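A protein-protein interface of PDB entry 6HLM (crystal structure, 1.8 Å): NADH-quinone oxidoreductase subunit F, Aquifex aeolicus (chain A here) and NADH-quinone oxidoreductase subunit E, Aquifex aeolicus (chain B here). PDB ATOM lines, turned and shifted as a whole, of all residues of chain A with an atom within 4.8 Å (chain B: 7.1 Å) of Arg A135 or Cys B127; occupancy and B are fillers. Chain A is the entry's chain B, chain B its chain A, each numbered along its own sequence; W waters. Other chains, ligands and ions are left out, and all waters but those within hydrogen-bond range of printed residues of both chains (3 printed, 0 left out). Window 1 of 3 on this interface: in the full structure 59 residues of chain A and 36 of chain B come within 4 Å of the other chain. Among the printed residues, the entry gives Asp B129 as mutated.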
ATOM      1  N   ALA A  93      -0.609  28.258  23.798  1.00  0.00           N
ATOM      2  CA  ALA A  93       0.305  29.391  23.588  1.00  0.00           C
ATOM      3  C   ALA A  93       1.723  28.851  23.419  1.00  0.00           C
ATOM      4  O   ALA A  93       2.699  29.542  23.759  1.00  0.00           O
ATOM      5  CB  ALA A  93       0.245  30.351  24.790  1.00  0.00           C
ATOM      6  N   ASP A  94       1.851  27.640  22.828  1.00  0.00           N
ATOM      7  CA  ASP A  94       3.171  27.056  22.648  1.00  0.00           C
ATOM      8  C   ASP A  94       3.962  27.681  21.512  1.00  0.00           C
ATOM      9  O   ASP A  94       5.174  27.515  21.475  1.00  0.00           O
ATOM     10  CB  ASP A  94       3.140  25.529  22.438  1.00  0.00           C
ATOM     11  CG  ASP A  94       4.511  24.935  22.784  1.00  0.00           C
ATOM     12  OD1 ASP A  94       4.972  25.127  23.939  1.00  0.00           O
ATOM     13  OD2 ASP A  94       5.167  24.405  21.883  1.00  0.00           O
ATOM     14  N   GLU A  95       3.264  28.329  20.557  1.00  0.00           N
ATOM     15  CA  GLU A  95       3.802  28.975  19.365  1.00  0.00           C
ATOM     16  C   GLU A  95       5.337  28.807  19.181  1.00  0.00           C
ATOM     17  O   GLU A  95       6.119  29.633  19.621  1.00  0.00           O
ATOM     18  CB  GLU A  95       3.379  30.451  19.388  1.00  0.00           C
ATOM     19  CG  GLU A  95       3.901  31.241  18.208  1.00  0.00           C
ATOM     20  CD  GLU A  95       3.231  32.580  18.077  1.00  0.00           C
ATOM     21  OE1 GLU A  95       3.590  33.509  18.838  1.00  0.00           O
ATOM     22  OE2 GLU A  95       2.362  32.706  17.182  1.00  0.00           O
ATOM     23  N   SER A  96       5.746  27.727  18.513  1.00  0.00           N
ATOM     24  CA  SER A  96       7.168  27.413  18.286  1.00  0.00           C
ATOM     25  C   SER A  96       7.480  27.107  16.832  1.00  0.00           C
ATOM     26  O   SER A  96       8.619  26.727  16.533  1.00  0.00           O
ATOM     27  CB  SER A  96       7.620  26.254  19.176  1.00  0.00           C
ATOM     28  OG  SER A  96       7.674  26.698  20.522  1.00  0.00           O
ATOM     29  N   GLU A  97       6.496  27.296  15.915  1.00  0.00           N
ATOM     30  CA  GLU A  97       6.787  27.026  14.493  1.00  0.00           C
ATOM     31  C   GLU A  97       7.615  28.180  13.919  1.00  0.00           C
ATOM     32  O   GLU A  97       7.220  29.331  14.127  1.00  0.00           O
ATOM     33  CB  GLU A  97       5.508  26.916  13.674  1.00  0.00           C
ATOM     34  CG  GLU A  97       5.822  26.193  12.375  1.00  0.00           C
ATOM     35  CD  GLU A  97       4.696  25.906  11.414  1.00  0.00           C
ATOM     36  OE1 GLU A  97       3.532  25.774  11.851  1.00  0.00           O
ATOM     37  OE2 GLU A  97       5.007  25.725  10.219  1.00  0.00           O
ATOM     38  N   PRO A  98       8.699  27.923  13.135  1.00  0.00           N
ATOM     39  CA  PRO A  98       9.470  29.037  12.550  1.00  0.00           C
ATOM     40  C   PRO A  98       8.593  30.012  11.762  1.00  0.00           C
ATOM     41  O   PRO A  98       7.662  29.602  11.040  1.00  0.00           O
ATOM     42  CB  PRO A  98      10.501  28.328  11.654  1.00  0.00           C
ATOM     43  CG  PRO A  98      10.692  27.002  12.291  1.00  0.00           C
ATOM     44  CD  PRO A  98       9.304  26.624  12.774  1.00  0.00           C
ATOM     45  N   GLY A  99       8.835  31.301  12.002  1.00  0.00           N
ATOM     46  CA  GLY A  99       8.112  32.388  11.350  1.00  0.00           C
ATOM     47  C   GLY A  99       6.811  32.804  11.998  1.00  0.00           C
ATOM     48  O   GLY A  99       6.271  33.859  11.639  1.00  0.00           O
ATOM     49  N   TYR A 133      -0.950  27.182  28.263  1.00  0.00           N
ATOM     50  CA  TYR A 133       0.336  26.504  28.208  1.00  0.00           C
ATOM     51  C   TYR A 133       1.189  27.376  27.297  1.00  0.00           C
ATOM     52  O   TYR A 133       0.901  27.477  26.121  1.00  0.00           O
ATOM     53  CB  TYR A 133       0.195  25.099  27.658  1.00  0.00           C
ATOM     54  CG  TYR A 133       1.487  24.317  27.688  1.00  0.00           C
ATOM     55  CD1 TYR A 133       2.417  24.430  26.655  1.00  0.00           C
ATOM     56  CD2 TYR A 133       1.777  23.453  28.741  1.00  0.00           C
ATOM     57  CE1 TYR A 133       3.582  23.671  26.650  1.00  0.00           C
ATOM     58  CE2 TYR A 133       2.961  22.714  28.766  1.00  0.00           C
ATOM     59  CZ  TYR A 133       3.856  22.820  27.712  1.00  0.00           C
ATOM     60  OH  TYR A 133       5.018  22.092  27.705  1.00  0.00           O
ATOM     61  N   ILE A 134       2.179  28.075  27.870  1.00  0.00           N
ATOM     62  CA  ILE A 134       3.007  29.005  27.086  1.00  0.00           C
ATOM     63  C   ILE A 134       4.410  28.441  26.974  1.00  0.00           C
ATOM     64  O   ILE A 134       4.934  27.949  27.970  1.00  0.00           O
ATOM     65  CB  ILE A 134       2.939  30.441  27.682  1.00  0.00           C
ATOM     66  CG1 ILE A 134       3.622  31.484  26.733  1.00  0.00           C
ATOM     67  CG2 ILE A 134       3.449  30.535  29.146  1.00  0.00           C
ATOM     68  CD1 ILE A 134       3.355  32.984  27.148  1.00  0.00           C
ATOM     69  N   ARG A 135       5.046  28.538  25.788  1.00  0.00           N
ATOM     70  CA  ARG A 135       6.414  28.003  25.657  1.00  0.00           C
ATOM     71  C   ARG A 135       7.370  28.668  26.671  1.00  0.00           C
ATOM     72  O   ARG A 135       7.141  29.830  27.051  1.00  0.00           O
ATOM     73  CB  ARG A 135       6.937  28.176  24.230  1.00  0.00           C
ATOM     74  CG  ARG A 135       7.156  29.645  23.835  1.00  0.00           C
ATOM     75  CD  ARG A 135       7.652  29.759  22.418  1.00  0.00           C
ATOM     76  NE  ARG A 135       8.998  29.204  22.243  1.00  0.00           N
ATOM     77  CZ  ARG A 135       9.680  29.312  21.113  1.00  0.00           C
ATOM     78  NH1 ARG A 135       9.147  29.932  20.067  1.00  0.00           N
ATOM     79  NH2 ARG A 135      10.911  28.827  21.027  1.00  0.00           N
ATOM     80  N   GLY A 136       8.394  27.927  27.107  1.00  0.00           N
ATOM     81  CA  GLY A 136       9.357  28.419  28.093  1.00  0.00           C
ATOM     82  C   GLY A 136      10.159  29.612  27.607  1.00  0.00           C
ATOM     83  O   GLY A 136      10.629  30.407  28.413  1.00  0.00           O
ATOM     84  N   GLU A 137      10.331  29.731  26.282  1.00  0.00           N
ATOM     85  CA  GLU A 137      11.076  30.844  25.645  1.00  0.00           C
ATOM     86  C   GLU A 137      10.268  32.122  25.503  1.00  0.00           C
ATOM     87  O   GLU A 137      10.788  33.114  24.972  1.00  0.00           O
ATOM     88  CB  GLU A 137      11.679  30.445  24.300  1.00  0.00           C
ATOM     89  CG  GLU A 137      12.581  29.216  24.367  1.00  0.00           C
ATOM     90  CD  GLU A 137      11.837  27.888  24.271  1.00  0.00           C
ATOM     91  OE1 GLU A 137      10.585  27.891  24.251  1.00  0.00           O
ATOM     92  OE2 GLU A 137      12.514  26.837  24.251  1.00  0.00           O
ATOM     93  N   TYR A 138       9.067  32.151  26.090  1.00  0.00           N
ATOM     94  CA  TYR A 138       8.270  33.375  26.193  1.00  0.00           C
ATOM     95  C   TYR A 138       8.202  33.747  27.685  1.00  0.00           C
ATOM     96  O   TYR A 138       7.107  33.745  28.258  1.00  0.00           O
ATOM     97  CB  TYR A 138       6.848  33.152  25.648  1.00  0.00           C
ATOM     98  CG  TYR A 138       6.659  33.155  24.146  1.00  0.00           C
ATOM     99  CD1 TYR A 138       7.703  33.504  23.282  1.00  0.00           C
ATOM    100  CD2 TYR A 138       5.431  32.828  23.585  1.00  0.00           C
ATOM    101  CE1 TYR A 138       7.513  33.534  21.896  1.00  0.00           C
ATOM    102  CE2 TYR A 138       5.238  32.845  22.207  1.00  0.00           C
ATOM    103  CZ  TYR A 138       6.268  33.229  21.371  1.00  0.00           C
ATOM    104  OH  TYR A 138       6.043  33.236  20.019  1.00  0.00           O
ATOM    105  N   GLY A 176       6.215  25.768  29.075  1.00  0.00           N
ATOM    106  CA  GLY A 176       6.936  24.749  28.330  1.00  0.00           C
ATOM    107  C   GLY A 176       8.396  24.819  28.735  1.00  0.00           C
ATOM    108  O   GLY A 176       8.782  25.633  29.598  1.00  0.00           O
ATOM    109  N   HIS B  35      12.649  25.127  36.023  1.00  0.00           N
ATOM    110  CA  HIS B  35      13.015  26.484  35.601  1.00  0.00           C
ATOM    111  C   HIS B  35      13.581  27.257  36.819  1.00  0.00           C
ATOM    112  O   HIS B  35      14.605  27.926  36.696  1.00  0.00           O
ATOM    113  CB  HIS B  35      11.806  27.254  35.020  1.00  0.00           C
ATOM    114  CG  HIS B  35      11.485  26.902  33.602  1.00  0.00           C
ATOM    115  ND1 HIS B  35      12.401  27.099  32.588  1.00  0.00           N
ATOM    116  CD2 HIS B  35      10.348  26.391  33.073  1.00  0.00           C
ATOM    117  CE1 HIS B  35      11.793  26.717  31.475  1.00  0.00           C
ATOM    118  NE2 HIS B  35      10.552  26.284  31.718  1.00  0.00           N
ATOM    119  N   MET B  72      15.532  23.251  27.240  1.00  0.00           N
ATOM    120  CA  MET B  72      15.977  24.397  28.044  1.00  0.00           C
ATOM    121  C   MET B  72      16.821  24.032  29.254  1.00  0.00           C
ATOM    122  O   MET B  72      17.613  24.869  29.697  1.00  0.00           O
ATOM    123  CB  MET B  72      14.782  25.265  28.471  1.00  0.00           C
ATOM    124  CG  MET B  72      14.185  26.069  27.301  1.00  0.00           C
ATOM    125  SD  MET B  72      12.874  27.193  27.849  1.00  0.00           S
ATOM    126  CE  MET B  72      13.870  28.502  28.654  1.00  0.00           C
ATOM    127  N   CYS B  86      19.339  32.103  18.215  1.00  0.00           N
ATOM    128  CA  CYS B  86      18.495  31.382  17.276  1.00  0.00           C
ATOM    129  C   CYS B  86      19.307  30.961  16.062  1.00  0.00           C
ATOM    130  O   CYS B  86      19.985  31.793  15.434  1.00  0.00           O
ATOM    131  CB  CYS B  86      17.267  32.183  16.862  1.00  0.00           C
ATOM    132  SG  CYS B  86      16.295  31.345  15.587  1.00  0.00           S
ATOM    133  N   VAL B  87      19.243  29.677  15.738  1.00  0.00           N
ATOM    134  CA  VAL B  87      19.980  29.126  14.593  1.00  0.00           C
ATOM    135  C   VAL B  87      18.994  28.616  13.520  1.00  0.00           C
ATOM    136  O   VAL B  87      19.384  27.863  12.622  1.00  0.00           O
ATOM    137  CB  VAL B  87      21.058  28.053  15.007  1.00  0.00           C
ATOM    138  CG1 VAL B  87      22.119  28.667  15.930  1.00  0.00           C
ATOM    139  CG2 VAL B  87      20.426  26.817  15.653  1.00  0.00           C
ATOM    140  N   SER B  88      17.720  29.016  13.624  1.00  0.00           N
ATOM    141  CA  SER B  88      16.696  28.595  12.647  1.00  0.00           C
ATOM    142  C   SER B  88      16.676  29.463  11.382  1.00  0.00           C
ATOM    143  O   SER B  88      17.469  30.390  11.252  1.00  0.00           O
ATOM    144  CB  SER B  88      15.314  28.500  13.281  1.00  0.00           C
ATOM    145  OG  SER B  88      15.330  27.434  14.208  1.00  0.00           O
ATOM    146  N   ILE B  89      15.758  29.140  10.461  1.00  0.00           N
ATOM    147  CA  ILE B  89      15.654  29.652   9.096  1.00  0.00           C
ATOM    148  C   ILE B  89      15.676  31.199   8.944  1.00  0.00           C
ATOM    149  O   ILE B  89      16.491  31.689   8.164  1.00  0.00           O
ATOM    150  CB  ILE B  89      14.432  29.030   8.337  1.00  0.00           C
ATOM    151  CG1 ILE B  89      14.259  29.613   6.902  1.00  0.00           C
ATOM    152  CG2 ILE B  89      13.126  29.161   9.123  1.00  0.00           C
ATOM    153  CD1 ILE B  89      15.313  29.277   5.941  1.00  0.00           C
ATOM    154  N   VAL B  90      14.768  31.947   9.586  1.00  0.00           N
ATOM    155  CA  VAL B  90      14.718  33.399   9.375  1.00  0.00           C
ATOM    156  C   VAL B  90      15.977  34.060   9.865  1.00  0.00           C
ATOM    157  O   VAL B  90      16.568  34.851   9.117  1.00  0.00           O
ATOM    158  CB  VAL B  90      13.435  34.075   9.918  1.00  0.00           C
ATOM    159  CG1 VAL B  90      13.264  35.477   9.341  1.00  0.00           C
ATOM    160  CG2 VAL B  90      12.206  33.225   9.610  1.00  0.00           C
ATOM    161  N   CYS B  91      16.418  33.733  11.098  1.00  0.00           N
ATOM    162  CA  CYS B  91      17.646  34.335  11.628  1.00  0.00           C
ATOM    163  C   CYS B  91      18.868  33.955  10.810  1.00  0.00           C
ATOM    164  O   CYS B  91      19.784  34.771  10.665  1.00  0.00           O
ATOM    165  CB  CYS B  91      17.818  34.049  13.112  1.00  0.00           C
ATOM    166  SG  CYS B  91      16.450  34.702  14.117  1.00  0.00           S
ATOM    167  N   VAL B 125      19.804  27.687  19.733  1.00  0.00           N
ATOM    168  CA  VAL B 125      18.398  27.264  19.916  1.00  0.00           C
ATOM    169  C   VAL B 125      17.578  27.332  18.628  1.00  0.00           C
ATOM    170  O   VAL B 125      17.939  28.059  17.692  1.00  0.00           O
ATOM    171  CB  VAL B 125      17.668  28.046  21.063  1.00  0.00           C
ATOM    172  CG1 VAL B 125      18.349  27.842  22.415  1.00  0.00           C
ATOM    173  CG2 VAL B 125      17.522  29.534  20.738  1.00  0.00           C
ATOM    174  N   GLN B 126      16.443  26.609  18.606  1.00  0.00           N
ATOM    175  CA  GLN B 126      15.511  26.667  17.484  1.00  0.00           C
ATOM    176  C   GLN B 126      14.709  27.984  17.574  1.00  0.00           C
ATOM    177  O   GLN B 126      14.777  28.675  18.589  1.00  0.00           O
ATOM    178  CB  GLN B 126      14.602  25.423  17.444  1.00  0.00           C
ATOM    179  CG  GLN B 126      15.377  24.119  17.127  1.00  0.00           C
ATOM    180  CD  GLN B 126      16.186  24.170  15.868  1.00  0.00           C
ATOM    181  OE1 GLN B 126      15.659  24.362  14.772  1.00  0.00           O
ATOM    182  NE2 GLN B 126      17.507  24.067  16.010  1.00  0.00           N
ATOM    183  N   CYS B 127      13.982  28.327  16.501  1.00  0.00           N
ATOM    184  CA  CYS B 127      13.179  29.563  16.374  1.00  0.00           C
ATOM    185  C   CYS B 127      12.549  30.037  17.676  1.00  0.00           C
ATOM    186  O   CYS B 127      11.794  29.311  18.315  1.00  0.00           O
ATOM    187  CB  CYS B 127      12.129  29.410  15.279  1.00  0.00           C
ATOM    188  SG  CYS B 127      11.102  30.880  15.044  1.00  0.00           S
ATOM    189  N   LEU B 128      12.885  31.279  18.061  1.00  0.00           N
ATOM    190  CA  LEU B 128      12.379  31.938  19.254  1.00  0.00           C
ATOM    191  C   LEU B 128      11.106  32.735  18.936  1.00  0.00           C
ATOM    192  O   LEU B 128      10.552  33.408  19.814  1.00  0.00           O
ATOM    193  CB  LEU B 128      13.481  32.868  19.809  1.00  0.00           C
ATOM    194  CG  LEU B 128      14.711  32.170  20.433  1.00  0.00           C
ATOM    195  CD1 LEU B 128      15.871  33.153  20.603  1.00  0.00           C
ATOM    196  CD2 LEU B 128      14.356  31.500  21.752  1.00  0.00           C
ATOM    197  N   ASP B 129      10.652  32.669  17.680  1.00  0.00           N
ATOM    198  CA  ASP B 129       9.476  33.351  17.165  1.00  0.00           C
ATOM    199  C   ASP B 129       9.436  34.861  17.473  1.00  0.00           C
ATOM    200  O   ASP B 129       8.476  35.372  18.031  1.00  0.00           O
ATOM    201  CB  ASP B 129       8.186  32.617  17.614  1.00  0.00           C
ATOM    202  CG  ASP B 129       8.039  31.345  16.816  1.00  0.00           C
ATOM    203  OD1 ASP B 129       7.827  31.444  15.590  1.00  0.00           O
ATOM    204  OD2 ASP B 129       8.302  30.270  17.372  1.00  0.00           O
ATOM    205  N   ALA B 130      10.517  35.566  17.102  1.00  0.00           N
ATOM    206  CA  ALA B 130      10.583  37.027  17.047  1.00  0.00           C
ATOM    207  C   ALA B 130      11.264  37.274  15.688  1.00  0.00           C
ATOM    208  O   ALA B 130      12.051  38.197  15.534  1.00  0.00           O
ATOM    209  CB  ALA B 130      11.395  37.606  18.205  1.00  0.00           C
ATOM    210  N   CYS B 131      10.913  36.427  14.689  1.00  0.00           N
ATOM    211  CA  CYS B 131      11.515  36.347  13.358  1.00  0.00           C
ATOM    212  C   CYS B 131      11.540  37.651  12.594  1.00  0.00           C
ATOM    213  O   CYS B 131      12.475  37.854  11.848  1.00  0.00           O
ATOM    214  CB  CYS B 131      10.879  35.244  12.511  1.00  0.00           C
ATOM    215  SG  CYS B 131      10.422  33.769  13.457  1.00  0.00           S
HETATM  216  O   HOH W   1      11.037  26.752  17.793  1.00  0.00           O
HETATM  217  O   HOH W   2      11.094  34.058  22.356  1.00  0.00           O
HETATM  218  O   HOH W   3      14.078  27.921  21.178  1.00  0.00           O
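A ring nitrogen (NE2) of His B35 sits at hydrogen-bond distance from the backbone carbonyl oxygen (O) of Gly A176 (2.8 Å). O of Cys B127 is in hydrogen-bond range of NH2 of Arg A135 (2.9 Å). O of Glu A97 lies close to OD1 of Asp B129. OD2 of Asp B129 is in salt-bridge range of NH1 of Arg A135. SG of Cys B131 lies close to N of Gly A99 (3.3 Å). O of Glu A95 sits close to OD2 of Asp B129, 3.2 Å away. OE2 of Glu A137 sits close to SD of Met B72 (3.6 Å).
The side-chain sulfur of Cys B127 lies close to the backbone NH of Asp B129. O of Asp A94 lies within hydrogen-bond range of OG of Ser A96 (2.8 Å). The guanidinium group (NE) of Arg A135 is in hydrogen-bond range of the side-chain hydroxyl (OG) of Ser A96 (3.3 Å). The backbone NH of Gly A176 sits at hydrogen-bond distance from the backbone carbonyl oxygen of Ile A134 (2.8 Å). The guanidinium group (NE) of Arg A135 is in salt-bridge range of the side-chain carboxylate (OE1) of Glu A137 (2.9 Å). The backbone NH (N) of Gly A136 sits close to the backbone carbonyl oxygen (O) of Gly A176 (3.4 Å).
Ser A96 touches Asp B129. Pro A98 touches Ile B89. CA of Pro A98 touches SG of Cys B127, at 3.5 Å. Cys B127 touches Gly A99 (SG to N, 3.8 Å). Asp B129 touches Gly A99 (OD1 to N, 3.7 Å). Arg A135 touches Leu B128. C of Gly A136 touches SD of Met B72, 3.6 Å away. Glu A137 touches Leu B128 (CB to CD2, 3.8 Å). Tyr A138 touches Leu B128. Tyr A138 touches Asp B129 (OH to CB, 3.3 Å).
Of the printed residues of chain B, Ser A96 touches Asp B129 (3.2 Å). Of chain B, only Cys B127 (2.9 Å), Leu B128 (3.6 Å) and Asp B129 (2.8 Å) come within 4 Å of Arg A135. Printed residues of chain B within 4 Å of Gly A176: His B35. Printed residues of chain A within 4 Å of His B35: Gly A176. Printed residues of chain A within 4 Å of Ile B89: Pro A98 (3.7 Å). Of chain A, only Pro A98 (3.5 Å), Gly A99 (3.8 Å) and Arg A135 (2.9 Å) come within 4 Å of Cys B127. Ala B130 touches none of the printed residues of chain A. Of the printed residues of chain A, Cys B131 touches Gly A99 (3.3 Å). The nearest residue of chain A that does not touch Cys B127 is Glu A97 (4.3 Å).
Of the 15 printed residues of chain B, 7 touch a printed residue of chain A. Hydrophobic or aromatic side chains of chain B that line the printed part of chain A: His B35, Met B72, Ile B89 and Leu B128. Along chain B the printed residues that touch a printed residue of chain A span positions 35 to 131.
Water W2 lies within hydrogen-bond range of O of Leu B128 (2.7 Å) and O of Glu A137 (2.8 Å). Water W1 bridges O of Cys B127 (2.7 Å) and O of Ser A96 (2.7 Å). Water W3 lies within hydrogen-bond range of O of Gln B126 (2.8 Å) and NH2 of Arg A135 (3.3 Å).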
